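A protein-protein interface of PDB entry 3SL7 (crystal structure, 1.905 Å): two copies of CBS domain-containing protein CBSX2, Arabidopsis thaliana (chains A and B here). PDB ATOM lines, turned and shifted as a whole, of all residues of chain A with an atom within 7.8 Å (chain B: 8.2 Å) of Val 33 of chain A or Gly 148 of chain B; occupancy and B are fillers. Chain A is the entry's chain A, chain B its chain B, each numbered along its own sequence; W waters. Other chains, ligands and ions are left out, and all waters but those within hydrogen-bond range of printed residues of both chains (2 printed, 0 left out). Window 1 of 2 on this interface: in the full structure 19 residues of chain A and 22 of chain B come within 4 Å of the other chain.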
ATOM      1  N   ASP A  26      27.310   3.594  -0.260  1.00  0.00           N
ATOM      2  CA  ASP A  26      26.345   2.753   0.445  1.00  0.00           C
ATOM      3  C   ASP A  26      26.254   1.369  -0.171  1.00  0.00           C
ATOM      4  O   ASP A  26      26.267   0.359   0.539  1.00  0.00           O
ATOM      5  CB  ASP A  26      24.948   3.399   0.441  1.00  0.00           C
ATOM      6  CG  ASP A  26      24.785   4.440   1.524  1.00  0.00           C
ATOM      7  OD1 ASP A  26      25.616   4.443   2.455  1.00  0.00           O
ATOM      8  OD2 ASP A  26      23.826   5.242   1.451  1.00  0.00           O
ATOM      9  N   ASP A  27      26.142   1.318  -1.495  1.00  0.00           N
ATOM     10  CA  ASP A  27      26.065   0.029  -2.169  1.00  0.00           C
ATOM     11  C   ASP A  27      27.355  -0.769  -2.034  1.00  0.00           C
ATOM     12  O   ASP A  27      27.311  -1.989  -1.895  1.00  0.00           O
ATOM     13  CB  ASP A  27      25.685   0.191  -3.636  1.00  0.00           C
ATOM     14  CG  ASP A  27      24.249   0.630  -3.812  1.00  0.00           C
ATOM     15  OD1 ASP A  27      23.454   0.511  -2.853  1.00  0.00           O
ATOM     16  OD2 ASP A  27      23.919   1.087  -4.921  1.00  0.00           O
ATOM     17  N   ALA A  28      28.498  -0.085  -2.086  1.00  0.00           N
ATOM     18  CA  ALA A  28      29.784  -0.740  -1.882  1.00  0.00           C
ATOM     19  C   ALA A  28      29.860  -1.311  -0.463  1.00  0.00           C
ATOM     20  O   ALA A  28      30.279  -2.448  -0.268  1.00  0.00           O
ATOM     21  CB  ALA A  28      30.924   0.235  -2.132  1.00  0.00           C
ATOM     22  N   LEU A  29      29.451  -0.523   0.526  1.00  0.00           N
ATOM     23  CA  LEU A  29      29.408  -1.008   1.904  1.00  0.00           C
ATOM     24  C   LEU A  29      28.516  -2.239   2.022  1.00  0.00           C
ATOM     25  O   LEU A  29      28.888  -3.219   2.662  1.00  0.00           O
ATOM     26  CB  LEU A  29      28.923   0.091   2.857  1.00  0.00           C
ATOM     27  CG  LEU A  29      29.950   1.160   3.218  1.00  0.00           C
ATOM     28  CD1 LEU A  29      29.293   2.322   3.968  1.00  0.00           C
ATOM     29  CD2 LEU A  29      31.089   0.570   4.021  1.00  0.00           C
ATOM     30  N   GLU A  30      27.342  -2.189   1.394  1.00  0.00           N
ATOM     31  CA  GLU A  30      26.407  -3.314   1.431  1.00  0.00           C
ATOM     32  C   GLU A  30      27.047  -4.576   0.844  1.00  0.00           C
ATOM     33  O   GLU A  30      26.907  -5.674   1.391  1.00  0.00           O
ATOM     34  CB  GLU A  30      25.113  -2.977   0.683  1.00  0.00           C
ATOM     35  CG  GLU A  30      23.933  -3.863   1.068  1.00  0.00           C
ATOM     36  CD  GLU A  30      22.642  -3.450   0.388  1.00  0.00           C
ATOM     37  OE1 GLU A  30      21.675  -4.243   0.417  1.00  0.00           O
ATOM     38  OE2 GLU A  30      22.593  -2.335  -0.174  1.00  0.00           O
ATOM     39  N   LEU A  31      27.744  -4.402  -0.273  1.00  0.00           N
ATOM     40  CA  LEU A  31      28.426  -5.505  -0.944  1.00  0.00           C
ATOM     41  C   LEU A  31      29.522  -6.074  -0.058  1.00  0.00           C
ATOM     42  O   LEU A  31      29.684  -7.297   0.037  1.00  0.00           O
ATOM     43  CB  LEU A  31      29.013  -5.038  -2.278  1.00  0.00           C
ATOM     44  CG  LEU A  31      29.609  -6.157  -3.135  1.00  0.00           C
ATOM     45  CD1 LEU A  31      28.539  -7.200  -3.437  1.00  0.00           C
ATOM     46  CD2 LEU A  31      30.183  -5.595  -4.421  1.00  0.00           C
ATOM     47  N   LEU A  32      30.283  -5.187   0.586  1.00  0.00           N
ATOM     48  CA  LEU A  32      31.310  -5.626   1.527  1.00  0.00           C
ATOM     49  C   LEU A  32      30.718  -6.529   2.590  1.00  0.00           C
ATOM     50  O   LEU A  32      31.230  -7.616   2.822  1.00  0.00           O
ATOM     51  CB  LEU A  32      31.980  -4.445   2.221  1.00  0.00           C
ATOM     52  CG  LEU A  32      33.002  -3.621   1.453  1.00  0.00           C
ATOM     53  CD1 LEU A  32      33.476  -2.485   2.341  1.00  0.00           C
ATOM     54  CD2 LEU A  32      34.169  -4.494   1.031  1.00  0.00           C
ATOM     55  N   VAL A  33      29.644  -6.077   3.233  1.00  0.00           N
ATOM     56  CA  VAL A  33      29.081  -6.800   4.371  1.00  0.00           C
ATOM     57  C   VAL A  33      28.340  -8.058   3.933  1.00  0.00           C
ATOM     58  O   VAL A  33      28.368  -9.066   4.629  1.00  0.00           O
ATOM     59  CB  VAL A  33      28.170  -5.904   5.283  1.00  0.00           C
ATOM     60  CG1 VAL A  33      28.899  -4.638   5.674  1.00  0.00           C
ATOM     61  CG2 VAL A  33      26.849  -5.582   4.603  1.00  0.00           C
ATOM     62  N   GLU A  34      27.689  -8.012   2.777  1.00  0.00           N
ATOM     63  CA  GLU A  34      27.004  -9.198   2.270  1.00  0.00           C
ATOM     64  C   GLU A  34      27.969 -10.287   1.804  1.00  0.00           C
ATOM     65  O   GLU A  34      27.751 -11.472   2.065  1.00  0.00           O
ATOM     66  CB  GLU A  34      26.027  -8.846   1.150  1.00  0.00           C
ATOM     67  CG  GLU A  34      24.590  -8.754   1.624  1.00  0.00           C
ATOM     68  CD  GLU A  34      23.614  -8.929   0.490  1.00  0.00           C
ATOM     69  OE1 GLU A  34      24.074  -9.028  -0.671  1.00  0.00           O
ATOM     70  OE2 GLU A  34      22.395  -8.974   0.760  1.00  0.00           O
ATOM     71  N   LYS A  35      29.033  -9.889   1.113  1.00  0.00           N
ATOM     72  CA  LYS A  35      30.000 -10.868   0.624  1.00  0.00           C
ATOM     73  C   LYS A  35      31.054 -11.173   1.684  1.00  0.00           C
ATOM     74  O   LYS A  35      31.884 -12.042   1.508  1.00  0.00           O
ATOM     75  CB  LYS A  35      30.643 -10.386  -0.667  1.00  0.00           C
ATOM     76  CG  LYS A  35      29.641 -10.148  -1.773  1.00  0.00           C
ATOM     77  CD  LYS A  35      28.733 -11.359  -1.958  1.00  0.00           C
ATOM     78  CE  LYS A  35      27.739 -11.112  -3.079  1.00  0.00           C
ATOM     79  NZ  LYS A  35      26.996 -12.343  -3.446  1.00  0.00           N
ATOM     80  N   LYS A  36      30.999 -10.451   2.797  1.00  0.00           N
ATOM     81  CA  LYS A  36      31.911 -10.673   3.911  1.00  0.00           C
ATOM     82  C   LYS A  36      33.367 -10.491   3.495  1.00  0.00           C
ATOM     83  O   LYS A  36      34.242 -11.281   3.833  1.00  0.00           O
ATOM     84  CB  LYS A  36      31.677 -12.044   4.560  1.00  0.00           C
ATOM     85  CG  LYS A  36      30.220 -12.297   4.955  1.00  0.00           C
ATOM     86  CD  LYS A  36      30.060 -13.600   5.732  1.00  0.00           C
ATOM     87  CE  LYS A  36      28.595 -13.940   5.996  1.00  0.00           C
ATOM     88  NZ  LYS A  36      27.877 -12.882   6.769  1.00  0.00           N
ATOM     89  N   VAL A  37      33.626  -9.431   2.750  1.00  0.00           N
ATOM     90  CA  VAL A  37      34.997  -9.045   2.455  1.00  0.00           C
ATOM     91  C   VAL A  37      35.251  -7.636   2.973  1.00  0.00           C
ATOM     92  O   VAL A  37      34.309  -6.905   3.282  1.00  0.00           O
ATOM     93  CB  VAL A  37      35.323  -9.141   0.945  1.00  0.00           C
ATOM     94  CG1 VAL A  37      35.200 -10.576   0.473  1.00  0.00           C
ATOM     95  CG2 VAL A  37      34.420  -8.239   0.128  1.00  0.00           C
ATOM     96  N   THR A  38      36.519  -7.253   3.069  1.00  0.00           N
ATOM     97  CA  THR A  38      36.849  -5.932   3.582  1.00  0.00           C
ATOM     98  C   THR A  38      37.379  -5.016   2.489  1.00  0.00           C
ATOM     99  O   THR A  38      37.628  -3.837   2.731  1.00  0.00           O
ATOM    100  CB  THR A  38      37.894  -6.009   4.692  1.00  0.00           C
ATOM    101  OG1 THR A  38      39.119  -6.513   4.145  1.00  0.00           O
ATOM    102  CG2 THR A  38      37.401  -6.921   5.813  1.00  0.00           C
ATOM    103  N   LEU A  40      37.448  -4.376  -2.111  1.00  0.00           N
ATOM    104  CA  LEU A  40      36.836  -4.681  -3.399  1.00  0.00           C
ATOM    105  C   LEU A  40      37.668  -4.112  -4.521  1.00  0.00           C
ATOM    106  O   LEU A  40      38.105  -2.959  -4.443  1.00  0.00           O
ATOM    107  CB  LEU A  40      35.460  -4.018  -3.483  1.00  0.00           C
ATOM    108  CG  LEU A  40      34.394  -4.402  -2.462  1.00  0.00           C
ATOM    109  CD1 LEU A  40      33.357  -3.284  -2.373  1.00  0.00           C
ATOM    110  CD2 LEU A  40      33.746  -5.721  -2.841  1.00  0.00           C
ATOM    111  N   ASP A  55      37.090  -1.125   3.207  1.00  0.00           N
ATOM    112  CA  ASP A  55      36.209  -0.607   4.252  1.00  0.00           C
ATOM    113  C   ASP A  55      36.804   0.650   4.899  1.00  0.00           C
ATOM    114  O   ASP A  55      36.081   1.592   5.180  1.00  0.00           O
ATOM    115  CB  ASP A  55      35.882  -1.673   5.311  1.00  0.00           C
ATOM    116  CG  ASP A  55      37.110  -2.452   5.775  1.00  0.00           C
ATOM    117  OD1 ASP A  55      38.254  -2.042   5.480  1.00  0.00           O
ATOM    118  OD2 ASP A  55      36.924  -3.481   6.454  1.00  0.00           O
ATOM    119  N   LEU A  59      34.658   4.165   5.053  1.00  0.00           N
ATOM    120  CA  LEU A  59      34.190   4.624   6.365  1.00  0.00           C
ATOM    121  C   LEU A  59      35.188   5.542   7.063  1.00  0.00           C
ATOM    122  O   LEU A  59      35.250   5.584   8.284  1.00  0.00           O
ATOM    123  CB  LEU A  59      33.867   3.429   7.266  1.00  0.00           C
ATOM    124  CG  LEU A  59      32.651   2.621   6.814  1.00  0.00           C
ATOM    125  CD1 LEU A  59      32.567   1.315   7.572  1.00  0.00           C
ATOM    126  CD2 LEU A  59      31.372   3.435   6.976  1.00  0.00           C
ATOM    127  N   TRP A  82      35.904   3.516  13.019  1.00  0.00           N
ATOM    128  CA  TRP A  82      34.867   3.755  14.023  1.00  0.00           C
ATOM    129  C   TRP A  82      35.099   2.887  15.257  1.00  0.00           C
ATOM    130  O   TRP A  82      35.528   1.737  15.144  1.00  0.00           O
ATOM    131  CB  TRP A  82      33.473   3.491  13.449  1.00  0.00           C
ATOM    132  CG  TRP A  82      33.281   2.105  12.895  1.00  0.00           C
ATOM    133  CD1 TRP A  82      33.606   1.678  11.642  1.00  0.00           C
ATOM    134  CD2 TRP A  82      32.715   0.969  13.569  1.00  0.00           C
ATOM    135  NE1 TRP A  82      33.282   0.351  11.489  1.00  0.00           N
ATOM    136  CE2 TRP A  82      32.733  -0.111  12.656  1.00  0.00           C
ATOM    137  CE3 TRP A  82      32.195   0.759  14.853  1.00  0.00           C
ATOM    138  CZ2 TRP A  82      32.250  -1.382  12.983  1.00  0.00           C
ATOM    139  CZ3 TRP A  82      31.714  -0.511  15.176  1.00  0.00           C
ATOM    140  CH2 TRP A  82      31.752  -1.563  14.242  1.00  0.00           C
ATOM    141  N   LEU A  88      29.900   5.062  14.160  1.00  0.00           N
ATOM    142  CA  LEU A  88      29.608   4.342  12.930  1.00  0.00           C
ATOM    143  C   LEU A  88      28.379   4.919  12.240  1.00  0.00           C
ATOM    144  O   LEU A  88      28.388   5.155  11.029  1.00  0.00           O
ATOM    145  CB  LEU A  88      29.393   2.860  13.223  1.00  0.00           C
ATOM    146  CG  LEU A  88      28.982   2.026  12.011  1.00  0.00           C
ATOM    147  CD1 LEU A  88      30.052   2.112  10.919  1.00  0.00           C
ATOM    148  CD2 LEU A  88      28.759   0.583  12.426  1.00  0.00           C
ATOM    149  N   PHE B   9      21.032  -8.638  14.328  1.00  0.00           N
ATOM    150  CA  PHE B   9      21.997  -8.473  13.241  1.00  0.00           C
ATOM    151  C   PHE B   9      23.153  -9.458  13.231  1.00  0.00           C
ATOM    152  O   PHE B   9      24.052  -9.357  12.401  1.00  0.00           O
ATOM    153  CB  PHE B   9      22.542  -7.048  13.251  1.00  0.00           C
ATOM    154  CG  PHE B   9      21.489  -6.006  13.025  1.00  0.00           C
ATOM    155  CD1 PHE B   9      21.083  -5.691  11.735  1.00  0.00           C
ATOM    156  CD2 PHE B   9      20.896  -5.355  14.090  1.00  0.00           C
ATOM    157  CE1 PHE B   9      20.104  -4.740  11.521  1.00  0.00           C
ATOM    158  CE2 PHE B   9      19.921  -4.398  13.883  1.00  0.00           C
ATOM    159  CZ  PHE B   9      19.522  -4.095  12.598  1.00  0.00           C
ATOM    160  N   THR B  11      25.383 -12.957  12.814  1.00  0.00           N
ATOM    161  CA  THR B  11      25.504 -14.052  11.864  1.00  0.00           C
ATOM    162  C   THR B  11      24.853 -15.267  12.493  1.00  0.00           C
ATOM    163  O   THR B  11      25.261 -15.700  13.569  1.00  0.00           O
ATOM    164  CB  THR B  11      26.967 -14.347  11.579  1.00  0.00           C
ATOM    165  OG1 THR B  11      27.611 -13.142  11.133  1.00  0.00           O
ATOM    166  CG2 THR B  11      27.113 -15.446  10.501  1.00  0.00           C
ATOM    167  N   LEU B 124      33.357  -5.418  20.342  1.00  0.00           N
ATOM    168  CA  LEU B 124      34.023  -5.971  19.173  1.00  0.00           C
ATOM    169  C   LEU B 124      35.459  -5.481  19.132  1.00  0.00           C
ATOM    170  O   LEU B 124      36.377  -6.219  18.791  1.00  0.00           O
ATOM    171  CB  LEU B 124      33.312  -5.533  17.898  1.00  0.00           C
ATOM    172  CG  LEU B 124      32.121  -6.360  17.464  1.00  0.00           C
ATOM    173  CD1 LEU B 124      31.543  -5.761  16.201  1.00  0.00           C
ATOM    174  CD2 LEU B 124      32.571  -7.792  17.220  1.00  0.00           C
ATOM    175  N   ARG B 130      38.112  -9.671  17.429  1.00  0.00           N
ATOM    176  CA  ARG B 130      37.330  -8.732  16.624  1.00  0.00           C
ATOM    177  C   ARG B 130      35.949  -9.253  16.216  1.00  0.00           C
ATOM    178  O   ARG B 130      35.308  -8.702  15.324  1.00  0.00           O
ATOM    179  CB  ARG B 130      38.118  -8.312  15.380  1.00  0.00           C
ATOM    180  CG  ARG B 130      39.358  -7.488  15.681  1.00  0.00           C
ATOM    181  CD  ARG B 130      38.989  -6.072  16.089  1.00  0.00           C
ATOM    182  NE  ARG B 130      39.948  -5.504  17.033  1.00  0.00           N
ATOM    183  CZ  ARG B 130      40.923  -4.668  16.694  1.00  0.00           C
ATOM    184  NH1 ARG B 130      41.075  -4.300  15.429  1.00  0.00           N
ATOM    185  NH2 ARG B 130      41.749  -4.200  17.620  1.00  0.00           N
ATOM    186  N   ARG B 131      35.499 -10.312  16.878  1.00  0.00           N
ATOM    187  CA  ARG B 131      34.161 -10.849  16.689  1.00  0.00           C
ATOM    188  C   ARG B 131      33.677 -11.254  18.072  1.00  0.00           C
ATOM    189  O   ARG B 131      34.481 -11.489  18.972  1.00  0.00           O
ATOM    190  CB  ARG B 131      34.170 -12.087  15.791  1.00  0.00           C
ATOM    191  CG  ARG B 131      34.977 -11.953  14.516  1.00  0.00           C
ATOM    192  CD  ARG B 131      35.186 -13.340  13.902  1.00  0.00           C
ATOM    193  NE  ARG B 131      35.898 -13.295  12.623  1.00  0.00           N
ATOM    194  CZ  ARG B 131      37.218 -13.235  12.509  1.00  0.00           C
ATOM    195  NH1 ARG B 131      37.974 -13.191  13.599  1.00  0.00           N
ATOM    196  NH2 ARG B 131      37.782 -13.219  11.305  1.00  0.00           N
ATOM    197  N   LEU B 145      28.798 -12.164  16.153  1.00  0.00           N
ATOM    198  CA  LEU B 145      28.688 -10.773  15.736  1.00  0.00           C
ATOM    199  C   LEU B 145      30.031 -10.326  15.205  1.00  0.00           C
ATOM    200  O   LEU B 145      31.033 -10.373  15.917  1.00  0.00           O
ATOM    201  CB  LEU B 145      28.244  -9.854  16.894  1.00  0.00           C
ATOM    202  CG  LEU B 145      27.992  -8.396  16.473  1.00  0.00           C
ATOM    203  CD1 LEU B 145      26.736  -8.292  15.612  1.00  0.00           C
ATOM    204  CD2 LEU B 145      27.870  -7.498  17.699  1.00  0.00           C
ATOM    205  N   THR B 146      30.042  -9.901  13.948  1.00  0.00           N
ATOM    206  CA  THR B 146      31.254  -9.436  13.304  1.00  0.00           C
ATOM    207  C   THR B 146      31.140  -7.936  13.100  1.00  0.00           C
ATOM    208  O   THR B 146      30.049  -7.386  13.181  1.00  0.00           O
ATOM    209  CB  THR B 146      31.408 -10.076  11.910  1.00  0.00           C
ATOM    210  OG1 THR B 146      30.419  -9.522  11.032  1.00  0.00           O
ATOM    211  CG2 THR B 146      31.247 -11.611  11.984  1.00  0.00           C
ATOM    212  N   ARG B 147      32.256  -7.280  12.800  1.00  0.00           N
ATOM    213  CA  ARG B 147      32.220  -5.865  12.452  1.00  0.00           C
ATOM    214  C   ARG B 147      31.325  -5.635  11.241  1.00  0.00           C
ATOM    215  O   ARG B 147      30.607  -4.634  11.175  1.00  0.00           O
ATOM    216  CB  ARG B 147      33.618  -5.319  12.194  1.00  0.00           C
ATOM    217  CG  ARG B 147      34.450  -5.164  13.441  1.00  0.00           C
ATOM    218  CD  ARG B 147      35.870  -4.744  13.106  1.00  0.00           C
ATOM    219  NE  ARG B 147      35.910  -3.544  12.270  1.00  0.00           N
ATOM    220  CZ  ARG B 147      35.693  -2.309  12.719  1.00  0.00           C
ATOM    221  NH1 ARG B 147      35.406  -2.106  13.999  1.00  0.00           N
ATOM    222  NH2 ARG B 147      35.755  -1.277  11.888  1.00  0.00           N
ATOM    223  N   GLY B 148      31.366  -6.570  10.294  1.00  0.00           N
ATOM    224  CA  GLY B 148      30.511  -6.509   9.125  1.00  0.00           C
ATOM    225  C   GLY B 148      29.038  -6.524   9.475  1.00  0.00           C
ATOM    226  O   GLY B 148      28.242  -5.820   8.855  1.00  0.00           O
ATOM    227  N   ASN B 149      28.665  -7.339  10.457  1.00  0.00           N
ATOM    228  CA  ASN B 149      27.283  -7.364  10.931  1.00  0.00           C
ATOM    229  C   ASN B 149      26.861  -6.006  11.485  1.00  0.00           C
ATOM    230  O   ASN B 149      25.733  -5.557  11.277  1.00  0.00           O
ATOM    231  CB  ASN B 149      27.091  -8.418  12.026  1.00  0.00           C
ATOM    232  CG  ASN B 149      27.246  -9.841  11.516  1.00  0.00           C
ATOM    233  OD1 ASN B 149      26.992 -10.139  10.345  1.00  0.00           O
ATOM    234  ND2 ASN B 149      27.654 -10.731  12.401  1.00  0.00           N
ATOM    235  N   VAL B 150      27.770  -5.361  12.205  1.00  0.00           N
ATOM    236  CA  VAL B 150      27.460  -4.083  12.838  1.00  0.00           C
ATOM    237  C   VAL B 150      27.326  -3.013  11.773  1.00  0.00           C
ATOM    238  O   VAL B 150      26.440  -2.182  11.851  1.00  0.00           O
ATOM    239  CB  VAL B 150      28.524  -3.680  13.865  1.00  0.00           C
ATOM    240  CG1 VAL B 150      28.230  -2.264  14.421  1.00  0.00           C
ATOM    241  CG2 VAL B 150      28.571  -4.714  14.992  1.00  0.00           C
ATOM    242  N   VAL B 151      28.191  -3.042  10.762  1.00  0.00           N
ATOM    243  CA  VAL B 151      28.053  -2.107   9.656  1.00  0.00           C
ATOM    244  C   VAL B 151      26.717  -2.327   8.940  1.00  0.00           C
ATOM    245  O   VAL B 151      26.020  -1.376   8.590  1.00  0.00           O
ATOM    246  CB  VAL B 151      29.216  -2.238   8.664  1.00  0.00           C
ATOM    247  CG1 VAL B 151      28.982  -1.348   7.455  1.00  0.00           C
ATOM    248  CG2 VAL B 151      30.530  -1.897   9.354  1.00  0.00           C
ATOM    249  N   ARG B 152      26.368  -3.589   8.718  1.00  0.00           N
ATOM    250  CA  ARG B 152      25.104  -3.924   8.079  1.00  0.00           C
ATOM    251  C   ARG B 152      23.939  -3.333   8.869  1.00  0.00           C
ATOM    252  O   ARG B 152      22.971  -2.839   8.292  1.00  0.00           O
ATOM    253  CB  ARG B 152      24.965  -5.439   7.959  1.00  0.00           C
ATOM    254  CG  ARG B 152      23.750  -5.913   7.195  1.00  0.00           C
ATOM    255  CD  ARG B 152      23.862  -7.410   6.947  1.00  0.00           C
ATOM    256  NE  ARG B 152      22.615  -7.981   6.457  1.00  0.00           N
ATOM    257  CZ  ARG B 152      21.594  -8.311   7.238  1.00  0.00           C
ATOM    258  NH1 ARG B 152      21.675  -8.123   8.549  1.00  0.00           N
ATOM    259  NH2 ARG B 152      20.491  -8.826   6.711  1.00  0.00           N
ATOM    260  N   ALA B 153      24.038  -3.371  10.193  1.00  0.00           N
ATOM    261  CA  ALA B 153      22.993  -2.807  11.041  1.00  0.00           C
ATOM    262  C   ALA B 153      22.868  -1.296  10.852  1.00  0.00           C
ATOM    263  O   ALA B 153      21.769  -0.779  10.649  1.00  0.00           O
ATOM    264  CB  ALA B 153      23.259  -3.136  12.496  1.00  0.00           C
ATOM    265  N   ALA B 154      23.988  -0.586  10.935  1.00  0.00           N
ATOM    266  CA  ALA B 154      23.983   0.857  10.710  1.00  0.00           C
ATOM    267  C   ALA B 154      23.361   1.199   9.353  1.00  0.00           C
ATOM    268  O   ALA B 154      22.582   2.151   9.242  1.00  0.00           O
ATOM    269  CB  ALA B 154      25.396   1.427  10.825  1.00  0.00           C
ATOM    270  N   LEU B 155      23.699   0.421   8.326  1.00  0.00           N
ATOM    271  CA  LEU B 155      23.148   0.642   6.992  1.00  0.00           C
ATOM    272  C   LEU B 155      21.644   0.442   6.956  1.00  0.00           C
ATOM    273  O   LEU B 155      20.914   1.258   6.393  1.00  0.00           O
ATOM    274  CB  LEU B 155      23.822  -0.284   5.970  1.00  0.00           C
ATOM    275  CG  LEU B 155      25.208   0.262   5.604  1.00  0.00           C
ATOM    276  CD1 LEU B 155      26.267  -0.772   5.235  1.00  0.00           C
ATOM    277  CD2 LEU B 155      25.197   1.485   4.685  1.00  0.00           C
ATOM    278  N   GLN B 156      21.187  -0.656   7.546  1.00  0.00           N
ATOM    279  CA  GLN B 156      19.772  -0.996   7.511  1.00  0.00           C
ATOM    280  C   GLN B 156      18.963   0.036   8.275  1.00  0.00           C
ATOM    281  O   GLN B 156      17.846   0.385   7.889  1.00  0.00           O
ATOM    282  CB  GLN B 156      19.545  -2.380   8.107  1.00  0.00           C
ATOM    283  CG  GLN B 156      18.085  -2.762   8.215  1.00  0.00           C
ATOM    284  CD  GLN B 156      17.886  -4.116   8.865  1.00  0.00           C
ATOM    285  OE1 GLN B 156      18.583  -5.082   8.547  1.00  0.00           O
ATOM    286  NE2 GLN B 156      16.933  -4.191   9.789  1.00  0.00           N
HETATM  287  O   HOH W   1      29.533 -13.027   9.034  1.00  0.00           O
HETATM  288  O   HOH W   2      34.352  -1.503   9.161  1.00  0.00           O
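The guanidinium group of Arg 147 of chain B sits close to the indole nitrogen of Trp 82 of chain A (3.0 Å).
The backbone NH of Gly 148 of chain B sits close to the side-chain hydroxyl of Thr 146 of chain B, 3.2 Å away.
Among the printed residues, merely in contact across the chains: Asp 26 of chain A with Leu 155 of chain B (3.7 Å), Leu 29 of chain A with Leu 155 of chain B (3.7 Å), Val 33 of chain A with Gly 148 of chain B (3.5 Å), Val 33 of chain A with Val 151 of chain B (3.7 Å), Val 33 of chain A with Arg 152 of chain B (3.9 Å), Trp 82 of chain A with Val 150 of chain B (3.6 Å), Leu 88 of chain A with Val 150 of chain B (3.5 Å), Leu 88 of chain A with Val 151 of chain B (3.9 Å) and Leu 88 of chain A with Ala 154 of chain B (3.8 Å).
Val 33 of chain A touches three residues of chain B.
Lys 35 of chain A touches none of the printed residues of chain B.
Printed residues of chain B within 4 Å of Trp 82 of chain A: Arg 147 (3.0 Å) and Val 150 (3.6 Å).
Gly 148 of chain B touches just one residue of chain A: Val 33.
Of the printed residues of chain A, Val 150 of chain B touches Trp 82 and Leu 88.
The nearest residue of chain B that does not touch Val 33 of chain A is Leu 155 of chain B (4.7 Å).
The nearest residue of chain A that does not touch Gly 148 of chain B is Trp 82 of chain A (5.9 Å).
Among the printed residues, 10 pairs touch across the chains.
Among the printed residues, no Asp or Glu carboxylate lies within 4 Å of a Lys or Arg side-chain nitrogen of the other chain.
No position is printed for both chains.
Of the 10 pairs that touch across the chains among the printed residues, none has its exchanged pair printed and touching as well.
Water W1 lies within hydrogen-bond range of NZ of Lys 36 of chain A and OG1 of Thr 11 of chain B.
Water W2 bridges the guanidinium group (NH2) of Arg 147 of chain B (3.1 Å) and the indole nitrogen (NE1) of Trp 82 of chain A (3.2 Å).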
